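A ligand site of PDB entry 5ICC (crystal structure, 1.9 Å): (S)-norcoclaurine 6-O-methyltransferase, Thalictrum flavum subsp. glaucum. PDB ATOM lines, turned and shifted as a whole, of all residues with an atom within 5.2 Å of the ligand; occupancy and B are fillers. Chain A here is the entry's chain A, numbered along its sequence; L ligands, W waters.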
ATOM      1  N   TRP A 151      12.353   8.195 -14.248  1.00  0.00           N
ATOM      2  CA  TRP A 151      11.550   6.951 -14.241  1.00  0.00           C
ATOM      3  C   TRP A 151      10.294   7.065 -15.118  1.00  0.00           C
ATOM      4  O   TRP A 151       9.970   6.125 -15.856  1.00  0.00           O
ATOM      5  CB  TRP A 151      11.171   6.544 -12.787  1.00  0.00           C
ATOM      6  CG  TRP A 151      12.440   6.565 -11.908  1.00  0.00           C
ATOM      7  CD1 TRP A 151      12.613   7.255 -10.765  1.00  0.00           C
ATOM      8  CD2 TRP A 151      13.692   5.929 -12.200  1.00  0.00           C
ATOM      9  NE1 TRP A 151      13.935   7.044 -10.263  1.00  0.00           N
ATOM     10  CE2 TRP A 151      14.597   6.241 -11.121  1.00  0.00           C
ATOM     11  CE3 TRP A 151      14.159   5.128 -13.249  1.00  0.00           C
ATOM     12  CZ2 TRP A 151      15.935   5.800 -11.090  1.00  0.00           C
ATOM     13  CZ3 TRP A 151      15.506   4.717 -13.220  1.00  0.00           C
ATOM     14  CH2 TRP A 151      16.369   5.034 -12.145  1.00  0.00           C
ATOM     15  N   PHE A 164      18.674   1.951 -21.319  1.00  0.00           N
ATOM     16  CA  PHE A 164      19.056   2.173 -19.942  1.00  0.00           C
ATOM     17  C   PHE A 164      19.111   0.835 -19.193  1.00  0.00           C
ATOM     18  O   PHE A 164      20.094   0.550 -18.440  1.00  0.00           O
ATOM     19  CB  PHE A 164      18.069   3.145 -19.264  1.00  0.00           C
ATOM     20  CG  PHE A 164      18.324   3.313 -17.815  1.00  0.00           C
ATOM     21  CD1 PHE A 164      19.237   4.272 -17.387  1.00  0.00           C
ATOM     22  CD2 PHE A 164      17.668   2.527 -16.868  1.00  0.00           C
ATOM     23  CE1 PHE A 164      19.494   4.457 -15.982  1.00  0.00           C
ATOM     24  CE2 PHE A 164      17.973   2.678 -15.464  1.00  0.00           C
ATOM     25  CZ  PHE A 164      18.859   3.665 -15.083  1.00  0.00           C
ATOM     26  N   ASN A 165      18.051   0.035 -19.329  1.00  0.00           N
ATOM     27  CA  ASN A 165      18.011  -1.250 -18.615  1.00  0.00           C
ATOM     28  C   ASN A 165      19.147  -2.156 -18.987  1.00  0.00           C
ATOM     29  O   ASN A 165      19.667  -2.906 -18.139  1.00  0.00           O
ATOM     30  CB  ASN A 165      16.660  -1.995 -18.824  1.00  0.00           C
ATOM     31  CG  ASN A 165      15.484  -1.236 -18.280  1.00  0.00           C
ATOM     32  OD1 ASN A 165      15.594  -0.462 -17.320  1.00  0.00           O
ATOM     33  ND2 ASN A 165      14.294  -1.497 -18.852  1.00  0.00           N
ATOM     34  N   MET A 168      22.333  -0.974 -17.205  1.00  0.00           N
ATOM     35  CA  MET A 168      22.346  -1.437 -15.798  1.00  0.00           C
ATOM     36  C   MET A 168      22.584  -2.966 -15.762  1.00  0.00           C
ATOM     37  O   MET A 168      23.272  -3.469 -14.865  1.00  0.00           O
ATOM     38  CB  MET A 168      21.009  -1.089 -15.119  1.00  0.00           C
ATOM     39  CG  MET A 168      20.770   0.445 -15.053  1.00  0.00           C
ATOM     40  SD  MET A 168      22.172   1.396 -14.385  1.00  0.00           S
ATOM     41  CE  MET A 168      22.519   0.633 -12.796  1.00  0.00           C
ATOM     42  N   ALA A 169      21.999  -3.702 -16.726  1.00  0.00           N
ATOM     43  CA  ALA A 169      22.277  -5.105 -16.827  1.00  0.00           C
ATOM     44  C   ALA A 169      23.785  -5.341 -16.971  1.00  0.00           C
ATOM     45  O   ALA A 169      24.347  -6.226 -16.297  1.00  0.00           O
ATOM     46  CB  ALA A 169      21.543  -5.736 -18.047  1.00  0.00           C
ATOM     47  N   THR A 172      25.678  -4.743 -13.748  1.00  0.00           N
ATOM     48  CA  THR A 172      25.447  -5.926 -12.878  1.00  0.00           C
ATOM     49  C   THR A 172      26.308  -7.121 -13.262  1.00  0.00           C
ATOM     50  O   THR A 172      26.943  -7.772 -12.385  1.00  0.00           O
ATOM     51  CB  THR A 172      23.900  -6.270 -12.916  1.00  0.00           C
ATOM     52  OG1 THR A 172      23.205  -5.147 -12.465  1.00  0.00           O
ATOM     53  CG2 THR A 172      23.588  -7.476 -11.930  1.00  0.00           C
ATOM     54  N   ASP A 195      15.007  -8.971  -5.087  1.00  0.00           N
ATOM     55  CA  ASP A 195      15.910  -7.896  -5.584  1.00  0.00           C
ATOM     56  C   ASP A 195      15.010  -6.690  -5.924  1.00  0.00           C
ATOM     57  O   ASP A 195      14.362  -6.662  -6.942  1.00  0.00           O
ATOM     58  CB  ASP A 195      16.684  -8.375  -6.793  1.00  0.00           C
ATOM     59  CG  ASP A 195      17.768  -7.389  -7.220  1.00  0.00           C
ATOM     60  OD1 ASP A 195      18.061  -6.435  -6.453  1.00  0.00           O
ATOM     61  OD2 ASP A 195      18.310  -7.563  -8.336  1.00  0.00           O
ATOM     62  N   VAL A 196      15.006  -5.723  -5.021  1.00  0.00           N
ATOM     63  CA  VAL A 196      14.111  -4.604  -5.101  1.00  0.00           C
ATOM     64  C   VAL A 196      14.682  -3.607  -6.083  1.00  0.00           C
ATOM     65  O   VAL A 196      15.859  -3.161  -5.944  1.00  0.00           O
ATOM     66  CB  VAL A 196      13.931  -3.976  -3.693  1.00  0.00           C
ATOM     67  CG1 VAL A 196      13.231  -2.561  -3.777  1.00  0.00           C
ATOM     68  CG2 VAL A 196      13.047  -4.900  -2.824  1.00  0.00           C
ATOM     69  N   GLY A 197      13.873  -3.234  -7.065  1.00  0.00           N
ATOM     70  CA  GLY A 197      14.374  -2.372  -8.173  1.00  0.00           C
ATOM     71  C   GLY A 197      15.353  -3.183  -8.986  1.00  0.00           C
ATOM     72  O   GLY A 197      16.358  -2.657  -9.486  1.00  0.00           O
ATOM     73  N   GLY A 198      15.077  -4.549  -9.067  1.00  0.00           N
ATOM     74  CA  GLY A 198      16.103  -5.518  -9.605  1.00  0.00           C
ATOM     75  C   GLY A 198      16.295  -5.449 -11.124  1.00  0.00           C
ATOM     76  O   GLY A 198      17.056  -6.274 -11.691  1.00  0.00           O
ATOM     77  N   GLY A 199      15.652  -4.429 -11.814  1.00  0.00           N
ATOM     78  CA  GLY A 199      15.919  -4.201 -13.230  1.00  0.00           C
ATOM     79  C   GLY A 199      15.350  -5.360 -14.033  1.00  0.00           C
ATOM     80  O   GLY A 199      14.294  -5.928 -13.668  1.00  0.00           O
ATOM     81  N   TYR A 219      11.803  -7.455  -8.502  1.00  0.00           N
ATOM     82  CA  TYR A 219      10.722  -6.518  -8.283  1.00  0.00           C
ATOM     83  C   TYR A 219      11.173  -5.169  -8.868  1.00  0.00           C
ATOM     84  O   TYR A 219      12.229  -4.656  -8.520  1.00  0.00           O
ATOM     85  CB  TYR A 219      10.520  -6.405  -6.758  1.00  0.00           C
ATOM     86  CG  TYR A 219       9.452  -5.418  -6.339  1.00  0.00           C
ATOM     87  CD1 TYR A 219       8.166  -5.526  -6.810  1.00  0.00           C
ATOM     88  CD2 TYR A 219       9.711  -4.451  -5.342  1.00  0.00           C
ATOM     89  CE1 TYR A 219       7.153  -4.623  -6.364  1.00  0.00           C
ATOM     90  CE2 TYR A 219       8.749  -3.586  -4.905  1.00  0.00           C
ATOM     91  CZ  TYR A 219       7.459  -3.680  -5.433  1.00  0.00           C
ATOM     92  OH  TYR A 219       6.486  -2.828  -4.982  1.00  0.00           O
ATOM     93  N   ASP A 220      10.345  -4.576  -9.727  1.00  0.00           N
ATOM     94  CA  ASP A 220      10.643  -3.270 -10.301  1.00  0.00           C
ATOM     95  C   ASP A 220       9.356  -2.631 -10.774  1.00  0.00           C
ATOM     96  O   ASP A 220       8.254  -3.218 -10.567  1.00  0.00           O
ATOM     97  CB  ASP A 220      11.643  -3.440 -11.475  1.00  0.00           C
ATOM     98  CG  ASP A 220      12.527  -2.194 -11.681  1.00  0.00           C
ATOM     99  OD1 ASP A 220      11.996  -1.118 -12.013  1.00  0.00           O
ATOM    100  OD2 ASP A 220      13.748  -2.300 -11.468  1.00  0.00           O
ATOM    101  N   LEU A 221       9.450  -1.479 -11.412  1.00  0.00           N
ATOM    102  CA  LEU A 221       8.241  -0.816 -11.968  1.00  0.00           C
ATOM    103  C   LEU A 221       7.708  -1.590 -13.143  1.00  0.00           C
ATOM    104  O   LEU A 221       8.475  -2.299 -13.853  1.00  0.00           O
ATOM    105  CB  LEU A 221       8.615   0.647 -12.415  1.00  0.00           C
ATOM    106  CG  LEU A 221       9.027   1.555 -11.244  1.00  0.00           C
ATOM    107  CD1 LEU A 221       9.724   2.819 -11.824  1.00  0.00           C
ATOM    108  CD2 LEU A 221       7.758   1.928 -10.427  1.00  0.00           C
ATOM    109  N   HIS A 223       6.963  -0.823 -16.236  1.00  0.00           N
ATOM    110  CA  HIS A 223       7.658  -0.644 -17.552  1.00  0.00           C
ATOM    111  C   HIS A 223       9.012  -1.315 -17.641  1.00  0.00           C
ATOM    112  O   HIS A 223       9.537  -1.538 -18.723  1.00  0.00           O
ATOM    113  CB  HIS A 223       7.730   0.846 -17.919  1.00  0.00           C
ATOM    114  CG  HIS A 223       8.537   1.680 -16.985  1.00  0.00           C
ATOM    115  ND1 HIS A 223       9.915   1.767 -17.050  1.00  0.00           N
ATOM    116  CD2 HIS A 223       8.177   2.422 -15.907  1.00  0.00           C
ATOM    117  CE1 HIS A 223      10.358   2.537 -16.078  1.00  0.00           C
ATOM    118  NE2 HIS A 223       9.329   2.944 -15.369  1.00  0.00           N
ATOM    119  N   VAL A 224       9.598  -1.667 -16.480  1.00  0.00           N
ATOM    120  CA  VAL A 224      10.856  -2.440 -16.496  1.00  0.00           C
ATOM    121  C   VAL A 224      10.580  -3.937 -16.555  1.00  0.00           C
ATOM    122  O   VAL A 224      11.253  -4.678 -17.301  1.00  0.00           O
ATOM    123  CB  VAL A 224      11.729  -2.064 -15.261  1.00  0.00           C
ATOM    124  CG1 VAL A 224      13.012  -2.960 -15.204  1.00  0.00           C
ATOM    125  CG2 VAL A 224      12.118  -0.607 -15.323  1.00  0.00           C
ATOM    126  N   GLY A 239       5.626  -3.212  -9.223  1.00  0.00           N
ATOM    127  CA  GLY A 239       5.020  -2.348  -8.204  1.00  0.00           C
ATOM    128  C   GLY A 239       5.851  -1.113  -7.879  1.00  0.00           C
ATOM    129  O   GLY A 239       6.759  -0.731  -8.649  1.00  0.00           O
ATOM    130  N   ASP A 240       5.525  -0.458  -6.779  1.00  0.00           N
ATOM    131  CA  ASP A 240       6.218   0.728  -6.353  1.00  0.00           C
ATOM    132  C   ASP A 240       6.818   0.452  -4.982  1.00  0.00           C
ATOM    133  O   ASP A 240       6.086   0.270  -3.982  1.00  0.00           O
ATOM    134  CB  ASP A 240       5.207   1.911  -6.315  1.00  0.00           C
ATOM    135  CG  ASP A 240       5.774   3.160  -5.727  1.00  0.00           C
ATOM    136  OD1 ASP A 240       6.985   3.275  -5.411  1.00  0.00           O
ATOM    137  OD2 ASP A 240       4.968   4.121  -5.576  1.00  0.00           O
ATOM    138  N   MET A 241       8.178   0.450  -4.910  1.00  0.00           N
ATOM    139  CA  MET A 241       8.890   0.091  -3.683  1.00  0.00           C
ATOM    140  C   MET A 241       8.614   1.054  -2.509  1.00  0.00           C
ATOM    141  O   MET A 241       8.824   0.698  -1.345  1.00  0.00           O
ATOM    142  CB  MET A 241      10.402  -0.013  -3.956  1.00  0.00           C
ATOM    143  CG  MET A 241      11.071   1.366  -4.159  1.00  0.00           C
ATOM    144  SD  MET A 241      12.762   1.174  -4.777  1.00  0.00           S
ATOM    145  CE  MET A 241      13.133   2.899  -5.212  1.00  0.00           C
ATOM    146  N   PHE A 242       8.157   2.269  -2.821  1.00  0.00           N
ATOM    147  CA  PHE A 242       7.790   3.222  -1.777  1.00  0.00           C
ATOM    148  C   PHE A 242       6.501   2.809  -1.108  1.00  0.00           C
ATOM    149  O   PHE A 242       6.253   3.235   0.034  1.00  0.00           O
ATOM    150  CB  PHE A 242       7.657   4.651  -2.327  1.00  0.00           C
ATOM    151  CG  PHE A 242       9.008   5.266  -2.590  1.00  0.00           C
ATOM    152  CD1 PHE A 242       9.705   5.878  -1.548  1.00  0.00           C
ATOM    153  CD2 PHE A 242       9.587   5.179  -3.858  1.00  0.00           C
ATOM    154  CE1 PHE A 242      11.007   6.428  -1.767  1.00  0.00           C
ATOM    155  CE2 PHE A 242      10.876   5.722  -4.078  1.00  0.00           C
ATOM    156  CZ  PHE A 242      11.568   6.345  -3.043  1.00  0.00           C
ATOM    157  N   LYS A 254      20.596  -3.098  -5.420  1.00  0.00           N
ATOM    158  CA  LYS A 254      21.813  -2.650  -6.082  1.00  0.00           C
ATOM    159  C   LYS A 254      21.538  -1.402  -6.898  1.00  0.00           C
ATOM    160  O   LYS A 254      20.587  -1.390  -7.683  1.00  0.00           O
ATOM    161  CB  LYS A 254      22.349  -3.755  -6.993  1.00  0.00           C
ATOM    162  CG  LYS A 254      23.573  -3.271  -7.849  1.00  0.00           C
ATOM    163  CD  LYS A 254      24.071  -4.426  -8.780  1.00  0.00           C
ATOM    164  CE  LYS A 254      25.092  -3.856  -9.710  1.00  0.00           C
ATOM    165  NZ  LYS A 254      24.514  -2.841 -10.695  1.00  0.00           N
ATOM    166  N   CYS A 255      22.360  -0.361  -6.718  1.00  0.00           N
ATOM    167  CA  CYS A 255      22.194   0.928  -7.451  1.00  0.00           C
ATOM    168  C   CYS A 255      20.772   1.457  -7.296  1.00  0.00           C
ATOM    169  O   CYS A 255      20.186   2.014  -8.237  1.00  0.00           O
ATOM    170  CB  CYS A 255      22.573   0.739  -8.938  1.00  0.00           C
ATOM    171  SG  CYS A 255      24.358   0.292  -9.119  1.00  0.00           S
ATOM    172  N   ILE A 256      20.255   1.359  -6.074  1.00  0.00           N
ATOM    173  CA  ILE A 256      18.905   1.899  -5.749  1.00  0.00           C
ATOM    174  C   ILE A 256      19.030   3.139  -4.893  1.00  0.00           C
ATOM    175  O   ILE A 256      18.598   4.197  -5.278  1.00  0.00           O
ATOM    176  CB  ILE A 256      18.010   0.851  -5.029  1.00  0.00           C
ATOM    177  CG1 ILE A 256      17.902  -0.449  -5.811  1.00  0.00           C
ATOM    178  CG2 ILE A 256      16.594   1.440  -4.656  1.00  0.00           C
ATOM    179  CD1 ILE A 256      17.388  -0.290  -7.317  1.00  0.00           C
ATOM    180  N   ASP A 259      20.049   6.557  -5.942  1.00  0.00           N
ATOM    181  CA  ASP A 259      19.050   7.364  -6.722  1.00  0.00           C
ATOM    182  C   ASP A 259      18.256   8.364  -5.930  1.00  0.00           C
ATOM    183  O   ASP A 259      17.520   9.209  -6.519  1.00  0.00           O
ATOM    184  CB  ASP A 259      18.054   6.442  -7.443  1.00  0.00           C
ATOM    185  CG  ASP A 259      18.697   5.552  -8.484  1.00  0.00           C
ATOM    186  OD1 ASP A 259      19.784   5.866  -9.043  1.00  0.00           O
ATOM    187  OD2 ASP A 259      18.079   4.490  -8.776  1.00  0.00           O
ATOM    188  N   TRP A 260      18.304   8.291  -4.616  1.00  0.00           N
ATOM    189  CA  TRP A 260      17.321   8.963  -3.777  1.00  0.00           C
ATOM    190  C   TRP A 260      18.044   9.792  -2.690  1.00  0.00           C
ATOM    191  O   TRP A 260      19.164   9.456  -2.290  1.00  0.00           O
ATOM    192  CB  TRP A 260      16.401   7.918  -3.077  1.00  0.00           C
ATOM    193  CG  TRP A 260      15.794   7.037  -4.077  1.00  0.00           C
ATOM    194  CD1 TRP A 260      16.178   5.779  -4.399  1.00  0.00           C
ATOM    195  CD2 TRP A 260      14.688   7.357  -4.911  1.00  0.00           C
ATOM    196  NE1 TRP A 260      15.402   5.296  -5.440  1.00  0.00           N
ATOM    197  CE2 TRP A 260      14.483   6.266  -5.777  1.00  0.00           C
ATOM    198  CE3 TRP A 260      13.859   8.472  -5.015  1.00  0.00           C
ATOM    199  CZ2 TRP A 260      13.448   6.244  -6.747  1.00  0.00           C
ATOM    200  CZ3 TRP A 260      12.825   8.453  -6.034  1.00  0.00           C
ATOM    201  CH2 TRP A 260      12.624   7.347  -6.844  1.00  0.00           C
HETATM  202  N1  LIG L   1      19.243  -2.995  -9.582  1.00  0.00           N
HETATM  203  C1  LIG L   1      19.484  -2.822 -11.048  1.00  0.00           C
HETATM  204  C2  LIG L   1      18.931  -1.482 -11.623  1.00  0.00           C
HETATM  205  C3  LIG L   1      19.411  -0.249 -10.853  1.00  0.00           C
HETATM  206  S1  LIG L   1      18.719   1.238 -11.656  1.00  0.00           S
HETATM  207  C4  LIG L   1      20.957  -2.795 -11.333  1.00  0.00           C
HETATM  208  O1  LIG L   1      21.772  -2.456 -10.461  1.00  0.00           O
HETATM  209  O2  LIG L   1      21.401  -3.172 -12.453  1.00  0.00           O
HETATM  210  C5  LIG L   1      17.449   1.682 -10.571  1.00  0.00           C
HETATM  211  C6  LIG L   1      16.206   0.773 -10.717  1.00  0.00           C
HETATM  212  O3  LIG L   1      15.231   1.220  -9.731  1.00  0.00           O
HETATM  213  C7  LIG L   1      15.515   0.958 -12.068  1.00  0.00           C
HETATM  214  O4  LIG L   1      15.357  -0.354 -12.672  1.00  0.00           O
HETATM  215  C8  LIG L   1      14.157   1.601 -11.789  1.00  0.00           C
HETATM  216  O5  LIG L   1      13.104   1.202 -12.668  1.00  0.00           O
HETATM  217  C9  LIG L   1      13.919   1.137 -10.377  1.00  0.00           C
HETATM  218  N2  LIG L   1      12.913   1.913  -9.625  1.00  0.00           N
HETATM  219  C10 LIG L   1      12.831   3.274  -9.582  1.00  0.00           C
HETATM  220  N3  LIG L   1      11.785   3.632  -8.840  1.00  0.00           N
HETATM  221  C11 LIG L   1      11.186   2.503  -8.396  1.00  0.00           C
HETATM  222  C12 LIG L   1      10.028   2.194  -7.555  1.00  0.00           C
HETATM  223  N4  LIG L   1       9.268   3.248  -7.028  1.00  0.00           N
HETATM  224  N5  LIG L   1       9.754   0.902  -7.299  1.00  0.00           N
HETATM  225  C13 LIG L   1      10.482  -0.136  -7.821  1.00  0.00           C
HETATM  226  N6  LIG L   1      11.559   0.111  -8.619  1.00  0.00           N
HETATM  227  C14 LIG L   1      11.921   1.373  -8.938  1.00  0.00           C
HETATM  228  O   HOH W   1      18.453  -3.854  -7.000  1.00  0.00           O
HETATM  229  O   HOH W   2      16.938  -1.161 -14.877  1.00  0.00           O
HETATM  230  O   HOH W   3      20.639   3.801 -10.599  1.00  0.00           O
HETATM  231  O   HOH W   4      19.990  -5.557  -9.338  1.00  0.00           O
HETATM  232  O   HOH W   5      12.922   2.722 -15.014  1.00  0.00           O
HETATM  233  O   HOH W   6       9.987   5.800  -8.776  1.00  0.00           O
HETATM  234  O   HOH W   7      19.878  -4.695 -14.086  1.00  0.00           O
HETATM  235  O   HOH W   8      15.660   3.400  -7.720  1.00  0.00           O
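An oxygen (O5) of the ligand is in hydrogen-bond range of the side-chain carboxylate of Asp 220 (2.7 Å). The side-chain hydroxyl (OG1) of Thr 172 sits at hydrogen-bond distance from an oxygen (O2) of the ligand (2.7 Å). The backbone carbonyl oxygen (O) of Lys 254 is in hydrogen-bond range of a nitrogen (N1) of the ligand (2.8 Å). The side-chain amino group (NZ) of Lys 254 lies within salt-bridge range of an oxygen (O1) of the ligand (2.8 Å). The side-chain carboxylate (OD1) of Asp 240 lies within hydrogen-bond range of a nitrogen (N4) of the ligand. A nitrogen (N5) of the ligand is in hydrogen-bond range of the backbone NH of Met 241. The backbone carbonyl oxygen (O) of Gly 197 lies within hydrogen-bond range of a nitrogen (N1) of the ligand, 2.9 Å away. O of Met 168 lies close to O2 of the ligand, 3.1 Å away.
The backbone NH (N) of Gly 239 sits at hydrogen-bond distance from the backbone carbonyl oxygen (O) of Asp 220, at 3.0 Å. N of Gly 199 sits at hydrogen-bond distance from OD2 of Asp 220. OG1 of Thr 172 sits at hydrogen-bond distance from NZ of Lys 254 (3.2 Å). The backbone carbonyl oxygen (O) of Met 168 is in hydrogen-bond range of the side-chain hydroxyl (OG1) of Thr 172. SG of Cys 255 is in hydrogen-bond range of NZ of Lys 254 (3.5 Å). The backbone NH of Phe 242 lies within hydrogen-bond range of the side-chain carboxylate of Asp 240 (3.0 Å). The backbone NH (N) of Gly 197 lies within hydrogen-bond range of the backbone carbonyl oxygen (O) of Tyr 219 (2.6 Å). O of Ile 256 lies close to NE1 of Trp 260 (3.4 Å).
Trp 151 touches the ligand. Gly 199 touches the ligand. CD2 of Leu 221 touches C12 of the ligand, 3.7 Å away. Val 224 touches the ligand (CG2 to O5, 3.4 Å). O of Gly 239 touches N5 of the ligand, at 3.7 Å. Phe 242 touches the ligand. Cys 255 touches the ligand. CD1 of Ile 256 touches O3 of the ligand, at 3.6 Å. OD2 of Asp 259 touches C5 of the ligand, 3.4 Å away. Trp 260 touches the ligand. Hydrophobic or aromatic side chains that line the ligand: Trp 151, Met 168, Leu 221, Val 224, Met 241, Phe 242, Ile 256 and Trp 260. The nearest printed residue that does not touch the ligand is Gly 198 (4.03 Å).
Water W4 lies within hydrogen-bond range of N1 of the ligand and OD2 of Asp 195. Water W2 lies within hydrogen-bond range of O4 of the ligand (2.8 Å) and OD1 of Asn 165 (2.9 Å). Water W8 lies within hydrogen-bond range of the side-chain carboxylate of Asp 259 (2.9 Å), the indole nitrogen of Trp 260 (3.0 Å) and an oxygen (O3) of the ligand (3.0 Å).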
